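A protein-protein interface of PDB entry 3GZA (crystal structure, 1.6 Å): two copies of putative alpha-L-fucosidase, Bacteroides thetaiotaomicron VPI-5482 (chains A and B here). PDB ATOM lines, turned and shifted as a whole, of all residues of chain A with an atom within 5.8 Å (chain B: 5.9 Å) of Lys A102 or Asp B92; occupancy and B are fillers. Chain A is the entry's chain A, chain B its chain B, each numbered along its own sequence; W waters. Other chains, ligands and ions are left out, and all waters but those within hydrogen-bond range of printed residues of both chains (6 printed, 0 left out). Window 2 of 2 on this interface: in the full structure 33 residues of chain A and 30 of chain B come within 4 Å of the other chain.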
ATOM      1  N   ASP A  50      29.861  -9.901  14.562  1.00  0.00           N
ATOM      2  CA  ASP A  50      28.646 -10.630  14.198  1.00  0.00           C
ATOM      3  C   ASP A  50      27.534 -10.231  15.098  1.00  0.00           C
ATOM      4  O   ASP A  50      27.519 -10.572  16.277  1.00  0.00           O
ATOM      5  CB  ASP A  50      28.969 -12.121  14.315  1.00  0.00           C
ATOM      6  CG  ASP A  50      27.798 -13.022  13.954  1.00  0.00           C
ATOM      7  OD1 ASP A  50      26.726 -12.515  13.611  1.00  0.00           O
ATOM      8  OD2 ASP A  50      27.984 -14.281  13.988  1.00  0.00           O
ATOM      9  N   TYR A  51      26.589  -9.489  14.565  1.00  0.00           N
ATOM     10  CA  TYR A  51      25.487  -9.051  15.383  1.00  0.00           C
ATOM     11  C   TYR A  51      24.489 -10.151  15.743  1.00  0.00           C
ATOM     12  O   TYR A  51      23.648  -9.950  16.630  1.00  0.00           O
ATOM     13  CB  TYR A  51      24.764  -7.857  14.788  1.00  0.00           C
ATOM     14  CG  TYR A  51      24.410  -7.934  13.304  1.00  0.00           C
ATOM     15  CD1 TYR A  51      23.328  -8.638  12.808  1.00  0.00           C
ATOM     16  CD2 TYR A  51      25.177  -7.189  12.399  1.00  0.00           C
ATOM     17  CE1 TYR A  51      23.042  -8.634  11.454  1.00  0.00           C
ATOM     18  CE2 TYR A  51      24.895  -7.164  11.070  1.00  0.00           C
ATOM     19  CZ  TYR A  51      23.836  -7.860  10.596  1.00  0.00           C
ATOM     20  OH  TYR A  51      23.602  -7.827   9.254  1.00  0.00           O
ATOM     21  N   ASN A  52      24.553 -11.325  15.110  1.00  0.00           N
ATOM     22  CA  ASN A  52      23.666 -12.409  15.485  1.00  0.00           C
ATOM     23  C   ASN A  52      24.025 -13.117  16.781  1.00  0.00           C
ATOM     24  O   ASN A  52      23.390 -14.090  17.175  1.00  0.00           O
ATOM     25  CB  ASN A  52      23.352 -13.351  14.322  1.00  0.00           C
ATOM     26  CG  ASN A  52      22.264 -12.754  13.431  1.00  0.00           C
ATOM     27  OD1 ASN A  52      21.168 -12.408  13.907  1.00  0.00           O
ATOM     28  ND2 ASN A  52      22.565 -12.603  12.147  1.00  0.00           N
ATOM     29  N   ALA A 100      17.591  -6.280  11.511  1.00  0.00           N
ATOM     30  CA  ALA A 100      18.702  -6.992  10.876  1.00  0.00           C
ATOM     31  C   ALA A 100      18.950  -8.384  11.370  1.00  0.00           C
ATOM     32  O   ALA A 100      19.636  -9.160  10.708  1.00  0.00           O
ATOM     33  CB  ALA A 100      19.989  -6.173  11.054  1.00  0.00           C
ATOM     34  N   VAL A 101      18.435  -8.698  12.564  1.00  0.00           N
ATOM     35  CA  VAL A 101      18.838  -9.897  13.248  1.00  0.00           C
ATOM     36  C   VAL A 101      17.863 -11.040  13.106  1.00  0.00           C
ATOM     37  O   VAL A 101      16.689 -10.831  12.769  1.00  0.00           O
ATOM     38  CB  VAL A 101      19.077  -9.632  14.767  1.00  0.00           C
ATOM     39  CG1 VAL A 101      20.141  -8.583  14.981  1.00  0.00           C
ATOM     40  CG2 VAL A 101      17.746  -9.312  15.499  1.00  0.00           C
ATOM     41  N   LYS A 102      18.358 -12.261  13.293  1.00  0.00           N
ATOM     42  CA  LYS A 102      17.514 -13.475  13.221  1.00  0.00           C
ATOM     43  C   LYS A 102      16.546 -13.617  14.399  1.00  0.00           C
ATOM     44  O   LYS A 102      15.423 -14.124  14.225  1.00  0.00           O
ATOM     45  CB  LYS A 102      18.399 -14.717  13.149  1.00  0.00           C
ATOM     46  CG  LYS A 102      19.277 -14.793  11.905  1.00  0.00           C
ATOM     47  CD  LYS A 102      20.299 -15.922  12.054  1.00  0.00           C
ATOM     48  CE  LYS A 102      21.193 -16.097  10.783  1.00  0.00           C
ATOM     49  NZ  LYS A 102      22.261 -17.205  10.890  1.00  0.00           N
ATOM     50  N   TRP A 103      16.970 -13.125  15.571  1.00  0.00           N
ATOM     51  CA  TRP A 103      16.130 -13.116  16.760  1.00  0.00           C
ATOM     52  C   TRP A 103      14.802 -12.426  16.459  1.00  0.00           C
ATOM     53  O   TRP A 103      14.765 -11.345  15.861  1.00  0.00           O
ATOM     54  CB  TRP A 103      16.859 -12.402  17.883  1.00  0.00           C
ATOM     55  CG  TRP A 103      16.086 -12.290  19.142  1.00  0.00           C
ATOM     56  CD1 TRP A 103      15.934 -13.248  20.079  1.00  0.00           C
ATOM     57  CD2 TRP A 103      15.395 -11.129  19.636  1.00  0.00           C
ATOM     58  NE1 TRP A 103      15.176 -12.772  21.127  1.00  0.00           N
ATOM     59  CE2 TRP A 103      14.847 -11.476  20.888  1.00  0.00           C
ATOM     60  CE3 TRP A 103      15.201  -9.837  19.158  1.00  0.00           C
ATOM     61  CZ2 TRP A 103      14.097 -10.576  21.655  1.00  0.00           C
ATOM     62  CZ3 TRP A 103      14.471  -8.961  19.915  1.00  0.00           C
ATOM     63  CH2 TRP A 103      13.939  -9.315  21.145  1.00  0.00           C
ATOM     64  N   ARG A 104      13.710 -13.091  16.850  1.00  0.00           N
ATOM     65  CA  ARG A 104      12.372 -12.609  16.577  1.00  0.00           C
ATOM     66  C   ARG A 104      12.079 -12.303  15.104  1.00  0.00           C
ATOM     67  O   ARG A 104      11.158 -11.541  14.794  1.00  0.00           O
ATOM     68  CB  ARG A 104      11.940 -11.480  17.512  1.00  0.00           C
ATOM     69  CG  ARG A 104      11.725 -11.978  18.933  1.00  0.00           C
ATOM     70  CD  ARG A 104      11.166 -10.890  19.791  1.00  0.00           C
ATOM     71  NE  ARG A 104      11.015 -11.376  21.166  1.00  0.00           N
ATOM     72  CZ  ARG A 104      10.601 -10.654  22.207  1.00  0.00           C
ATOM     73  NH1 ARG A 104      10.256  -9.390  22.090  1.00  0.00           N
ATOM     74  NH2 ARG A 104      10.551 -11.237  23.395  1.00  0.00           N
ATOM     75  N   ASP A 105      12.797 -12.997  14.216  1.00  0.00           N
ATOM     76  CA  ASP A 105      12.574 -12.946  12.777  1.00  0.00           C
ATOM     77  C   ASP A 105      12.629 -11.516  12.255  1.00  0.00           C
ATOM     78  O   ASP A 105      11.896 -11.159  11.309  1.00  0.00           O
ATOM     79  CB  ASP A 105      11.224 -13.629  12.471  1.00  0.00           C
ATOM     80  CG  ASP A 105      11.011 -13.947  10.979  1.00  0.00           C
ATOM     81  OD1 ASP A 105      11.988 -14.220  10.247  1.00  0.00           O
ATOM     82  OD2 ASP A 105       9.844 -13.935  10.568  1.00  0.00           O
ATOM     83  N   GLY A 106      13.494 -10.731  12.880  1.00  0.00           N
ATOM     84  CA  GLY A 106      13.659  -9.330  12.511  1.00  0.00           C
ATOM     85  C   GLY A 106      12.515  -8.390  12.808  1.00  0.00           C
ATOM     86  O   GLY A 106      12.487  -7.257  12.300  1.00  0.00           O
ATOM     87  N   TRP B  89      19.656  -8.486  -1.125  1.00  0.00           N
ATOM     88  CA  TRP B  89      19.364  -9.809  -0.632  1.00  0.00           C
ATOM     89  C   TRP B  89      19.159  -9.751   0.874  1.00  0.00           C
ATOM     90  O   TRP B  89      19.305  -8.713   1.519  1.00  0.00           O
ATOM     91  CB  TRP B  89      20.461 -10.804  -1.056  1.00  0.00           C
ATOM     92  CG  TRP B  89      21.756 -10.777  -0.303  1.00  0.00           C
ATOM     93  CD1 TRP B  89      22.142 -11.667   0.647  1.00  0.00           C
ATOM     94  CD2 TRP B  89      22.844  -9.837  -0.441  1.00  0.00           C
ATOM     95  NE1 TRP B  89      23.392 -11.360   1.123  1.00  0.00           N
ATOM     96  CE2 TRP B  89      23.833 -10.217   0.496  1.00  0.00           C
ATOM     97  CE3 TRP B  89      23.068  -8.686  -1.224  1.00  0.00           C
ATOM     98  CZ2 TRP B  89      25.030  -9.543   0.623  1.00  0.00           C
ATOM     99  CZ3 TRP B  89      24.264  -8.015  -1.068  1.00  0.00           C
ATOM    100  CH2 TRP B  89      25.237  -8.468  -0.176  1.00  0.00           C
ATOM    101  N   GLN B  90      18.768 -10.900   1.405  1.00  0.00           N
ATOM    102  CA  GLN B  90      18.609 -11.114   2.835  1.00  0.00           C
ATOM    103  C   GLN B  90      19.943 -11.485   3.456  1.00  0.00           C
ATOM    104  O   GLN B  90      20.297 -12.669   3.585  1.00  0.00           O
ATOM    105  CB  GLN B  90      17.573 -12.186   3.052  1.00  0.00           C
ATOM    106  CG  GLN B  90      16.113 -11.777   2.687  1.00  0.00           C
ATOM    107  CD  GLN B  90      15.471 -10.936   3.784  1.00  0.00           C
ATOM    108  OE1 GLN B  90      15.510 -11.324   4.988  1.00  0.00           O
ATOM    109  NE2 GLN B  90      14.910  -9.797   3.401  1.00  0.00           N
ATOM    110  N   SER B  91      20.697 -10.458   3.800  1.00  0.00           N
ATOM    111  CA  SER B  91      22.010 -10.657   4.393  1.00  0.00           C
ATOM    112  C   SER B  91      21.905 -10.740   5.909  1.00  0.00           C
ATOM    113  O   SER B  91      21.054 -10.102   6.525  1.00  0.00           O
ATOM    114  CB  SER B  91      22.955  -9.538   4.016  1.00  0.00           C
ATOM    115  OG  SER B  91      24.271  -9.770   4.487  1.00  0.00           O
ATOM    116  N   ASP B  92      22.816 -11.516   6.466  1.00  0.00           N
ATOM    117  CA  ASP B  92      22.984 -11.667   7.922  1.00  0.00           C
ATOM    118  C   ASP B  92      24.263 -10.954   8.424  1.00  0.00           C
ATOM    119  O   ASP B  92      24.589 -11.019   9.614  1.00  0.00           O
ATOM    120  CB  ASP B  92      22.982 -13.148   8.298  1.00  0.00           C
ATOM    121  CG  ASP B  92      21.704 -13.822   7.931  1.00  0.00           C
ATOM    122  OD1 ASP B  92      20.599 -13.313   8.223  1.00  0.00           O
ATOM    123  OD2 ASP B  92      21.760 -14.924   7.309  1.00  0.00           O
ATOM    124  N   VAL B  93      24.943 -10.226   7.518  1.00  0.00           N
ATOM    125  CA  VAL B  93      26.175  -9.514   7.827  1.00  0.00           C
ATOM    126  C   VAL B  93      26.115  -8.031   7.428  1.00  0.00           C
ATOM    127  O   VAL B  93      26.725  -7.140   8.078  1.00  0.00           O
ATOM    128  CB  VAL B  93      27.418 -10.168   7.232  1.00  0.00           C
ATOM    129  CG1 VAL B  93      27.546 -11.605   7.711  1.00  0.00           C
ATOM    130  CG2 VAL B  93      27.416 -10.126   5.689  1.00  0.00           C
ATOM    131  N   ASN B  94      25.426  -7.745   6.323  1.00  0.00           N
ATOM    132  CA  ASN B  94      25.194  -6.382   5.923  1.00  0.00           C
ATOM    133  C   ASN B  94      23.783  -6.004   6.299  1.00  0.00           C
ATOM    134  O   ASN B  94      22.850  -6.461   5.669  1.00  0.00           O
ATOM    135  CB  ASN B  94      25.406  -6.235   4.413  1.00  0.00           C
ATOM    136  CG  ASN B  94      25.051  -4.842   3.908  1.00  0.00           C
ATOM    137  OD1 ASN B  94      24.923  -3.889   4.702  1.00  0.00           O
ATOM    138  ND2 ASN B  94      24.966  -4.696   2.560  1.00  0.00           N
ATOM    139  N   CYS B  97      20.297  -3.773   3.892  1.00  0.00           N
ATOM    140  CA  CYS B  97      19.873  -4.722   2.861  1.00  0.00           C
ATOM    141  C   CYS B  97      18.363  -4.727   2.900  1.00  0.00           C
ATOM    142  O   CYS B  97      17.735  -3.877   3.550  1.00  0.00           O
ATOM    143  CB  CYS B  97      20.484  -6.107   3.054  1.00  0.00           C
ATOM    144  SG  CYS B  97      19.808  -7.042   4.451  1.00  0.00           S
ATOM    145  N   LYS B  99      16.310  -6.379   4.387  1.00  0.00           N
ATOM    146  CA  LYS B  99      15.692  -6.512   5.729  1.00  0.00           C
ATOM    147  C   LYS B  99      15.308  -5.151   6.325  1.00  0.00           C
ATOM    148  O   LYS B  99      14.433  -5.093   7.192  1.00  0.00           O
ATOM    149  CB  LYS B  99      16.670  -7.194   6.675  1.00  0.00           C
ATOM    150  CG  LYS B  99      16.904  -8.706   6.404  1.00  0.00           C
ATOM    151  CD  LYS B  99      17.884  -9.269   7.420  1.00  0.00           C
ATOM    152  CE  LYS B  99      18.095 -10.738   7.213  1.00  0.00           C
ATOM    153  NZ  LYS B  99      16.823 -11.482   7.511  1.00  0.00           N
ATOM    154  N   GLU B 168      28.159 -15.312   1.534  1.00  0.00           N
ATOM    155  CA  GLU B 168      26.707 -15.475   1.460  1.00  0.00           C
ATOM    156  C   GLU B 168      26.273 -15.661   0.005  1.00  0.00           C
ATOM    157  O   GLU B 168      25.523 -16.534  -0.337  1.00  0.00           O
ATOM    158  CB  GLU B 168      26.021 -14.228   2.017  1.00  0.00           C
ATOM    159  CG  GLU B 168      26.048 -14.144   3.544  1.00  0.00           C
ATOM    160  CD  GLU B 168      25.252 -12.983   4.095  1.00  0.00           C
ATOM    161  OE1 GLU B 168      25.003 -12.006   3.341  1.00  0.00           O
ATOM    162  OE2 GLU B 168      24.941 -12.997   5.329  1.00  0.00           O
ATOM    163  N   ARG B 172      24.436 -19.372  -1.049  1.00  0.00           N
ATOM    164  CA  ARG B 172      22.993 -19.458  -0.820  1.00  0.00           C
ATOM    165  C   ARG B 172      22.135 -19.372  -2.074  1.00  0.00           C
ATOM    166  O   ARG B 172      20.894 -19.545  -1.986  1.00  0.00           O
ATOM    167  CB  ARG B 172      22.569 -18.305   0.111  1.00  0.00           C
ATOM    168  CG  ARG B 172      23.270 -18.271   1.465  1.00  0.00           C
ATOM    169  CD  ARG B 172      22.836 -17.112   2.283  1.00  0.00           C
ATOM    170  NE  ARG B 172      23.452 -17.140   3.599  1.00  0.00           N
ATOM    171  CZ  ARG B 172      23.111 -16.315   4.583  1.00  0.00           C
ATOM    172  NH1 ARG B 172      22.191 -15.378   4.379  1.00  0.00           N
ATOM    173  NH2 ARG B 172      23.684 -16.436   5.748  1.00  0.00           N
HETATM  174  O   HOH W   1      21.118  -8.270   8.519  1.00  0.00           O
HETATM  175  O   HOH W   2      25.363 -13.100  11.257  1.00  0.00           O
HETATM  176  O   HOH W   3      26.876  -9.840  11.425  1.00  0.00           O
HETATM  177  O   HOH W   4      16.019 -10.270  10.207  1.00  0.00           O
HETATM  178  O   HOH W   5      20.494 -11.789  10.449  1.00  0.00           O
HETATM  179  O   HOH W   6      24.206 -16.862   9.145  1.00  0.00           O
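Among the printed residues, pairs that only touch across the chains: Asn A52 with Asp B92, Ala A100 with Lys B99 and Lys A102 with Asp B92.
Lys A102 touches just one residue of chain B: Asp B92 (3.7 Å). Asp B92 touches just these residues of chain A: Tyr A51 (3.3 Å), Asn A52 (3.6 Å) and Lys A102 (3.7 Å). Of the printed residues of chain B, Asn A52 touches Asp B92 (3.6 Å). Of the printed residues of chain A, Val B93 touches Tyr A51. Val A101 touches none of the printed residues of chain B. The nearest residue of chain A that does not touch Asp B92 is Asp A50 (4.8 Å).
The side-chain hydroxyl (OH) of Tyr A51 sits at hydrogen-bond distance from the backbone NH (N) of Asn B94, at 3.5 Å. The side-chain hydroxyl of Tyr A51 lies close to the backbone NH of Val B93 (3.3 Å). The side-chain hydroxyl (OH) of Tyr A51 lies close to the backbone carbonyl oxygen (O) of Asp B92 (3.4 Å).
OD2 of Asp B92 lies within salt-bridge range of NH2 of Arg B172, 2.9 Å away. The side-chain amide oxygen (OD1) of Asn A52 sits at hydrogen-bond distance from the backbone NH (N) of Lys A102. The side-chain amino group of Lys B99 lies within hydrogen-bond range of the side-chain amide oxygen of Gln B90 (2.8 Å). N of Asn B94 is in hydrogen-bond range of OG of Ser B91 (3.0 Å). The side-chain carboxylate of Asp A50 is in hydrogen-bond range of the backbone NH of Asn A52 (2.9 Å). The side-chain sulfur (SG) of Cys B97 sits close to the backbone NH (N) of Lys B99.
No position is printed for both chains.
Water W1 lies within hydrogen-bond range of OH of Tyr A51 (2.6 Å), O of Ser B91 (2.7 Å) and O of Ala A100 (2.8 Å). Water W6 bridges NZ of Lys A102 and NH2 of Arg B172. Water W5 lies within hydrogen-bond range of the side-chain carboxylate of Asp B92 (2.7 Å), the backbone carbonyl oxygen of Ala A100 (2.8 Å) and the side-chain amide nitrogen of Asn A52 (2.8 Å). Water W4 bridges the backbone carbonyl oxygen (O) of Val A101 and the side-chain amino group (NZ) of Lys B99. Water W2 lies within hydrogen-bond range of O of Asp B92 (2.8 Å), OD1 of Asp A50 (2.8 Å) and ND2 of Asn A52 (3.0 Å). Water W3 lies within hydrogen-bond range of O of Asp B92, N of Tyr A51 and OD1 of Asp A50.
Of the 10 printed residues of chain B, 4 touch a printed residue of chain A. Printed residues of chain B that touch a printed residue of chain A: Asp B92, Val B93, Asn B94 and Lys B99. Hydrophobic or aromatic side chains of chain A within 4 Å of the printed part of chain B: Tyr A51. Among the printed residues, 6 pairs touch across the chains. Among the printed residues, no Asp or Glu carboxylate lies within 4 Å of a Lys or Arg side-chain nitrogen of the other chain.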
